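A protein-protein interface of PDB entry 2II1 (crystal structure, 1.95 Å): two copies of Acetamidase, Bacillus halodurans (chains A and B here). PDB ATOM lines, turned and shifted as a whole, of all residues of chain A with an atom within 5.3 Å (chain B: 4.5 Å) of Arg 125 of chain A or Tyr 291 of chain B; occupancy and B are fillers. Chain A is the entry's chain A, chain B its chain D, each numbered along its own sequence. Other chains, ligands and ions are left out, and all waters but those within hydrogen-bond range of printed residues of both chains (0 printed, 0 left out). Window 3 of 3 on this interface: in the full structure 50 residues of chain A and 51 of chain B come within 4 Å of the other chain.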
ATOM      1  N   GLU A 114     -22.066   4.312 -18.622  1.00  0.00           N
ATOM      2  CA  GLU A 114     -23.455   3.905 -18.472  1.00  0.00           C
ATOM      3  C   GLU A 114     -23.496   2.534 -17.821  1.00  0.00           C
ATOM      4  O   GLU A 114     -23.020   1.564 -18.411  1.00  0.00           O
ATOM      5  CB  GLU A 114     -24.077   3.845 -19.863  1.00  0.00           C
ATOM      6  CG  GLU A 114     -25.551   4.053 -19.960  1.00  0.00           C
ATOM      7  CD  GLU A 114     -25.947   4.160 -21.408  1.00  0.00           C
ATOM      8  OE1 GLU A 114     -25.812   5.271 -21.979  1.00  0.00           O
ATOM      9  OE2 GLU A 114     -26.310   3.116 -21.992  1.00  0.00           O
ATOM     10  N   ASP A 117     -20.510  -0.002 -17.953  1.00  0.00           N
ATOM     11  CA  ASP A 117     -19.960   0.020 -19.337  1.00  0.00           C
ATOM     12  C   ASP A 117     -19.324   1.358 -19.721  1.00  0.00           C
ATOM     13  O   ASP A 117     -19.802   2.411 -19.294  1.00  0.00           O
ATOM     14  CB  ASP A 117     -21.077  -0.274 -20.372  1.00  0.00           C
ATOM     15  CG  ASP A 117     -21.722  -1.646 -20.187  1.00  0.00           C
ATOM     16  OD1 ASP A 117     -20.993  -2.640 -19.986  1.00  0.00           O
ATOM     17  OD2 ASP A 117     -22.958  -1.742 -20.245  1.00  0.00           O
ATOM     18  N   VAL A 118     -18.257   1.320 -20.523  1.00  0.00           N
ATOM     19  CA  VAL A 118     -17.777   2.498 -21.271  1.00  0.00           C
ATOM     20  C   VAL A 118     -18.391   2.454 -22.691  1.00  0.00           C
ATOM     21  O   VAL A 118     -18.152   1.516 -23.477  1.00  0.00           O
ATOM     22  CB  VAL A 118     -16.215   2.588 -21.339  1.00  0.00           C
ATOM     23  CG1 VAL A 118     -15.763   3.785 -22.178  1.00  0.00           C
ATOM     24  CG2 VAL A 118     -15.569   2.634 -19.936  1.00  0.00           C
ATOM     25  N   VAL A 119     -19.214   3.448 -23.017  1.00  0.00           N
ATOM     26  CA  VAL A 119     -19.890   3.451 -24.304  1.00  0.00           C
ATOM     27  C   VAL A 119     -18.961   3.996 -25.412  1.00  0.00           C
ATOM     28  O   VAL A 119     -18.657   5.198 -25.430  1.00  0.00           O
ATOM     29  CB  VAL A 119     -21.235   4.233 -24.247  1.00  0.00           C
ATOM     30  CG1 VAL A 119     -21.923   4.213 -25.636  1.00  0.00           C
ATOM     31  CG2 VAL A 119     -22.172   3.612 -23.210  1.00  0.00           C
ATOM     32  N   TYR A 120     -18.512   3.106 -26.306  1.00  0.00           N
ATOM     33  CA  TYR A 120     -17.627   3.462 -27.433  1.00  0.00           C
ATOM     34  C   TYR A 120     -18.445   3.918 -28.650  1.00  0.00           C
ATOM     35  O   TYR A 120     -18.151   4.933 -29.273  1.00  0.00           O
ATOM     36  CB  TYR A 120     -16.724   2.258 -27.786  1.00  0.00           C
ATOM     37  CG  TYR A 120     -15.746   2.444 -28.945  1.00  0.00           C
ATOM     38  CD1 TYR A 120     -16.173   2.366 -30.285  1.00  0.00           C
ATOM     39  CD2 TYR A 120     -14.383   2.638 -28.709  1.00  0.00           C
ATOM     40  CE1 TYR A 120     -15.253   2.521 -31.360  1.00  0.00           C
ATOM     41  CE2 TYR A 120     -13.475   2.800 -29.757  1.00  0.00           C
ATOM     42  CZ  TYR A 120     -13.914   2.749 -31.081  1.00  0.00           C
ATOM     43  OH  TYR A 120     -13.000   2.882 -32.103  1.00  0.00           O
ATOM     44  N   SER A 121     -19.467   3.144 -28.975  1.00  0.00           N
ATOM     45  CA  SER A 121     -20.388   3.441 -30.058  1.00  0.00           C
ATOM     46  C   SER A 121     -21.686   2.664 -29.812  1.00  0.00           C
ATOM     47  O   SER A 121     -21.807   1.917 -28.816  1.00  0.00           O
ATOM     48  CB  SER A 121     -19.796   3.045 -31.406  1.00  0.00           C
ATOM     49  OG  SER A 121     -19.552   1.651 -31.437  1.00  0.00           O
ATOM     50  N   GLY A 123     -22.766   0.110 -31.291  1.00  0.00           N
ATOM     51  CA  GLY A 123     -22.480  -1.325 -31.299  1.00  0.00           C
ATOM     52  C   GLY A 123     -21.424  -1.846 -30.338  1.00  0.00           C
ATOM     53  O   GLY A 123     -21.438  -3.028 -30.025  1.00  0.00           O
ATOM     54  N   LEU A 124     -20.515  -0.989 -29.868  1.00  0.00           N
ATOM     55  CA  LEU A 124     -19.378  -1.421 -29.026  1.00  0.00           C
ATOM     56  C   LEU A 124     -19.417  -0.816 -27.613  1.00  0.00           C
ATOM     57  O   LEU A 124     -19.605   0.374 -27.439  1.00  0.00           O
ATOM     58  CB  LEU A 124     -18.033  -1.057 -29.673  1.00  0.00           C
ATOM     59  CG  LEU A 124     -17.433  -1.880 -30.822  1.00  0.00           C
ATOM     60  CD1 LEU A 124     -16.126  -1.255 -31.333  1.00  0.00           C
ATOM     61  CD2 LEU A 124     -17.187  -3.308 -30.392  1.00  0.00           C
ATOM     62  N   ARG A 125     -19.213  -1.656 -26.612  1.00  0.00           N
ATOM     63  CA  ARG A 125     -19.167  -1.214 -25.228  1.00  0.00           C
ATOM     64  C   ARG A 125     -17.991  -1.888 -24.549  1.00  0.00           C
ATOM     65  O   ARG A 125     -17.699  -3.067 -24.802  1.00  0.00           O
ATOM     66  CB  ARG A 125     -20.472  -1.556 -24.508  1.00  0.00           C
ATOM     67  CG  ARG A 125     -21.663  -0.794 -25.030  1.00  0.00           C
ATOM     68  CD  ARG A 125     -22.994  -1.383 -24.551  1.00  0.00           C
ATOM     69  NE  ARG A 125     -23.368  -0.991 -23.186  1.00  0.00           N
ATOM     70  CZ  ARG A 125     -24.050   0.107 -22.854  1.00  0.00           C
ATOM     71  NH1 ARG A 125     -24.434   0.983 -23.773  1.00  0.00           N
ATOM     72  NH2 ARG A 125     -24.333   0.350 -21.580  1.00  0.00           N
ATOM     73  N   LEU A 126     -17.298  -1.128 -23.714  1.00  0.00           N
ATOM     74  CA  LEU A 126     -16.187  -1.684 -22.949  1.00  0.00           C
ATOM     75  C   LEU A 126     -16.574  -1.837 -21.492  1.00  0.00           C
ATOM     76  O   LEU A 126     -17.390  -1.094 -20.983  1.00  0.00           O
ATOM     77  CB  LEU A 126     -14.935  -0.819 -23.074  1.00  0.00           C
ATOM     78  CG  LEU A 126     -14.548  -0.273 -24.450  1.00  0.00           C
ATOM     79  CD1 LEU A 126     -13.154   0.305 -24.411  1.00  0.00           C
ATOM     80  CD2 LEU A 126     -14.650  -1.334 -25.541  1.00  0.00           C
ATOM     81  N   PRO A 127     -15.972  -2.810 -20.808  1.00  0.00           N
ATOM     82  CA  PRO A 127     -16.237  -2.920 -19.386  1.00  0.00           C
ATOM     83  C   PRO A 127     -15.660  -1.737 -18.650  1.00  0.00           C
ATOM     84  O   PRO A 127     -14.578  -1.264 -18.991  1.00  0.00           O
ATOM     85  CB  PRO A 127     -15.533  -4.229 -18.968  1.00  0.00           C
ATOM     86  CG  PRO A 127     -15.005  -4.836 -20.208  1.00  0.00           C
ATOM     87  CD  PRO A 127     -15.023  -3.823 -21.297  1.00  0.00           C
ATOM     88  N   ALA B 268      -9.160  -1.333 -24.797  1.00  0.00           N
ATOM     89  CA  ALA B 268      -9.700  -2.687 -24.676  1.00  0.00           C
ATOM     90  C   ALA B 268      -8.700  -3.770 -25.088  1.00  0.00           C
ATOM     91  O   ALA B 268      -8.937  -4.927 -24.812  1.00  0.00           O
ATOM     92  CB  ALA B 268     -10.993  -2.815 -25.558  1.00  0.00           C
ATOM     93  N   LEU B 287      -6.574  -8.721 -28.778  1.00  0.00           N
ATOM     94  CA  LEU B 287      -7.920  -8.143 -28.708  1.00  0.00           C
ATOM     95  C   LEU B 287      -8.993  -9.249 -28.682  1.00  0.00           C
ATOM     96  O   LEU B 287      -8.984 -10.187 -29.490  1.00  0.00           O
ATOM     97  CB  LEU B 287      -8.152  -7.173 -29.870  1.00  0.00           C
ATOM     98  CG  LEU B 287      -9.397  -6.276 -29.770  1.00  0.00           C
ATOM     99  CD1 LEU B 287      -9.332  -5.312 -28.563  1.00  0.00           C
ATOM    100  CD2 LEU B 287      -9.597  -5.514 -31.074  1.00  0.00           C
ATOM    101  N   ALA B 288      -9.932  -9.145 -27.751  1.00  0.00           N
ATOM    102  CA  ALA B 288     -10.976 -10.128 -27.634  1.00  0.00           C
ATOM    103  C   ALA B 288     -11.742 -10.337 -28.958  1.00  0.00           C
ATOM    104  O   ALA B 288     -12.052  -9.380 -29.683  1.00  0.00           O
ATOM    105  CB  ALA B 288     -11.959  -9.737 -26.499  1.00  0.00           C
ATOM    106  N   LEU B 289     -12.077 -11.593 -29.260  1.00  0.00           N
ATOM    107  CA  LEU B 289     -12.834 -11.909 -30.474  1.00  0.00           C
ATOM    108  C   LEU B 289     -14.241 -11.275 -30.452  1.00  0.00           C
ATOM    109  O   LEU B 289     -14.801 -10.918 -31.506  1.00  0.00           O
ATOM    110  CB  LEU B 289     -12.935 -13.422 -30.646  1.00  0.00           C
ATOM    111  CG  LEU B 289     -11.674 -14.265 -30.881  1.00  0.00           C
ATOM    112  CD1 LEU B 289     -11.981 -15.730 -30.701  1.00  0.00           C
ATOM    113  CD2 LEU B 289     -11.053 -14.024 -32.265  1.00  0.00           C
ATOM    114  N   HIS B 290     -14.803 -11.143 -29.247  1.00  0.00           N
ATOM    115  CA  HIS B 290     -16.045 -10.392 -28.998  1.00  0.00           C
ATOM    116  C   HIS B 290     -16.147  -9.097 -29.823  1.00  0.00           C
ATOM    117  O   HIS B 290     -17.170  -8.825 -30.447  1.00  0.00           O
ATOM    118  CB  HIS B 290     -16.148 -10.068 -27.494  1.00  0.00           C
ATOM    119  CG  HIS B 290     -17.197  -9.058 -27.168  1.00  0.00           C
ATOM    120  ND1 HIS B 290     -16.893  -7.774 -26.772  1.00  0.00           N
ATOM    121  CD2 HIS B 290     -18.551  -9.127 -27.228  1.00  0.00           C
ATOM    122  CE1 HIS B 290     -18.016  -7.099 -26.584  1.00  0.00           C
ATOM    123  NE2 HIS B 290     -19.035  -7.895 -26.861  1.00  0.00           N
ATOM    124  N   TYR B 291     -15.070  -8.318 -29.841  1.00  0.00           N
ATOM    125  CA  TYR B 291     -15.050  -7.044 -30.575  1.00  0.00           C
ATOM    126  C   TYR B 291     -15.033  -7.232 -32.109  1.00  0.00           C
ATOM    127  O   TYR B 291     -15.723  -6.519 -32.845  1.00  0.00           O
ATOM    128  CB  TYR B 291     -13.869  -6.170 -30.106  1.00  0.00           C
ATOM    129  CG  TYR B 291     -13.928  -5.797 -28.632  1.00  0.00           C
ATOM    130  CD1 TYR B 291     -14.944  -4.985 -28.133  1.00  0.00           C
ATOM    131  CD2 TYR B 291     -12.950  -6.258 -27.731  1.00  0.00           C
ATOM    132  CE1 TYR B 291     -14.999  -4.645 -26.773  1.00  0.00           C
ATOM    133  CE2 TYR B 291     -12.986  -5.926 -26.381  1.00  0.00           C
ATOM    134  CZ  TYR B 291     -14.012  -5.119 -25.902  1.00  0.00           C
ATOM    135  OH  TYR B 291     -14.053  -4.798 -24.565  1.00  0.00           O
ATOM    136  N   PHE B 292     -14.262  -8.203 -32.588  1.00  0.00           N
ATOM    137  CA  PHE B 292     -14.242  -8.521 -34.018  1.00  0.00           C
ATOM    138  C   PHE B 292     -15.630  -8.926 -34.543  1.00  0.00           C
ATOM    139  O   PHE B 292     -16.012  -8.595 -35.673  1.00  0.00           O
ATOM    140  CB  PHE B 292     -13.246  -9.634 -34.299  1.00  0.00           C
ATOM    141  CG  PHE B 292     -11.831  -9.216 -34.146  1.00  0.00           C
ATOM    142  CD1 PHE B 292     -11.202  -8.497 -35.145  1.00  0.00           C
ATOM    143  CD2 PHE B 292     -11.120  -9.524 -32.997  1.00  0.00           C
ATOM    144  CE1 PHE B 292      -9.897  -8.113 -35.004  1.00  0.00           C
ATOM    145  CE2 PHE B 292      -9.817  -9.139 -32.852  1.00  0.00           C
ATOM    146  CZ  PHE B 292      -9.197  -8.443 -33.861  1.00  0.00           C
ATOM    147  N   GLU B 293     -16.381  -9.645 -33.717  1.00  0.00           N
ATOM    148  CA  GLU B 293     -17.710 -10.112 -34.094  1.00  0.00           C
ATOM    149  C   GLU B 293     -18.662  -8.909 -34.113  1.00  0.00           C
ATOM    150  O   GLU B 293     -19.413  -8.731 -35.051  1.00  0.00           O
ATOM    151  CB  GLU B 293     -18.188 -11.220 -33.142  1.00  0.00           C
ATOM    152  CG  GLU B 293     -17.209 -12.444 -32.997  1.00  0.00           C
ATOM    153  CD  GLU B 293     -16.909 -13.190 -34.314  1.00  0.00           C
ATOM    154  OE1 GLU B 293     -17.834 -13.338 -35.157  1.00  0.00           O
ATOM    155  OE2 GLU B 293     -15.746 -13.649 -34.495  1.00  0.00           O
ATOM    156  N   LYS B 294     -18.590  -8.070 -33.082  1.00  0.00           N
ATOM    157  CA  LYS B 294     -19.321  -6.794 -33.037  1.00  0.00           C
ATOM    158  C   LYS B 294     -19.035  -5.850 -34.227  1.00  0.00           C
ATOM    159  O   LYS B 294     -19.911  -5.070 -34.613  1.00  0.00           O
ATOM    160  CB  LYS B 294     -19.023  -6.059 -31.726  1.00  0.00           C
ATOM    161  CG  LYS B 294     -19.892  -6.463 -30.551  1.00  0.00           C
ATOM    162  CD  LYS B 294     -19.425  -5.712 -29.310  1.00  0.00           C
ATOM    163  CE  LYS B 294     -20.517  -5.529 -28.246  1.00  0.00           C
ATOM    164  NZ  LYS B 294     -20.073  -4.568 -27.159  1.00  0.00           N
ATOM    165  N   LEU B 295     -17.824  -5.905 -34.786  1.00  0.00           N
ATOM    166  CA  LEU B 295     -17.467  -5.122 -35.985  1.00  0.00           C
ATOM    167  C   LEU B 295     -17.667  -5.935 -37.283  1.00  0.00           C
ATOM    168  O   LEU B 295     -17.225  -5.519 -38.367  1.00  0.00           O
ATOM    169  CB  LEU B 295     -16.020  -4.609 -35.890  1.00  0.00           C
ATOM    170  CG  LEU B 295     -15.681  -3.559 -34.816  1.00  0.00           C
ATOM    171  CD1 LEU B 295     -14.164  -3.510 -34.585  1.00  0.00           C
ATOM    172  CD2 LEU B 295     -16.207  -2.164 -35.168  1.00  0.00           C
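The side-chain carboxylate (OD2) of Asp 117 of chain A lies within salt-bridge range of the guanidinium group (NH2) of Arg 125 of chain A. N of Leu 124 of chain A is in hydrogen-bond range of OG of Ser 121 of chain A, at 3.2 Å. The backbone carbonyl oxygen of Leu 126 of chain A lies within hydrogen-bond range of the backbone NH of Val 118 of chain A (2.6 Å). NE2 of His 290 of chain B sits close to NZ of Lys 294 of chain B, 3.5 Å away. The side-chain carboxylate (OE2) of Glu 114 of chain A lies within salt-bridge range of the guanidinium group (NH1) of Arg 125 of chain A, 3.4 Å away.
The backbone NH (N) of Arg 125 of chain A sits close to the side-chain amino group (NZ) of Lys 294 of chain B, 3.1 Å away.
Hydrophobic or aromatic side chains of chain B that line the printed part of chain A: Ala 268, Tyr 291 and Leu 295. Along chain B the printed residues that touch a printed residue of chain A span positions 268 to 295. Of the 11 printed residues of chain A, 5 touch a printed residue of chain B.
Among the printed residues, merely in contact across the chains: Gly 123 of chain A with Lys 294 of chain B (3.2 Å), Leu 124 of chain A with Lys 294 of chain B (3.5 Å), Pro 127 of chain A with Tyr 291 of chain B (3.5 Å), Leu 126 of chain A with Tyr 291 of chain B (3.5 Å), Leu 124 of chain A with Tyr 291 of chain B (3.6 Å), Arg 125 of chain A with Tyr 291 of chain B (3.7 Å), Leu 124 of chain A with Leu 295 of chain B (3.9 Å) and Leu 126 of chain A with Ala 268 of chain B (3.9 Å).
No position is printed for both chains.
Printed residues of chain B within 4 Å of Gly 123 of chain A: Lys 294 (3.2 Å). Of the printed residues of chain B, Leu 124 of chain A touches Tyr 291, Lys 294 and Leu 295. Printed residues of chain B within 4 Å of Arg 125 of chain A: Tyr 291 and Lys 294. Printed residues of chain B within 4 Å of Pro 127 of chain A: Tyr 291. Of the printed residues of chain A, Ala 268 of chain B touches Leu 126. Tyr 291 of chain B touches just these residues of chain A: Leu 124, Arg 125, Leu 126 and Pro 127. Of the printed residues of chain A, Lys 294 of chain B touches Gly 123, Leu 124 and Arg 125. The nearest printed residue of chain B that does not touch Pro 127 of chain A is Ala 268 of chain B (6.0 Å).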
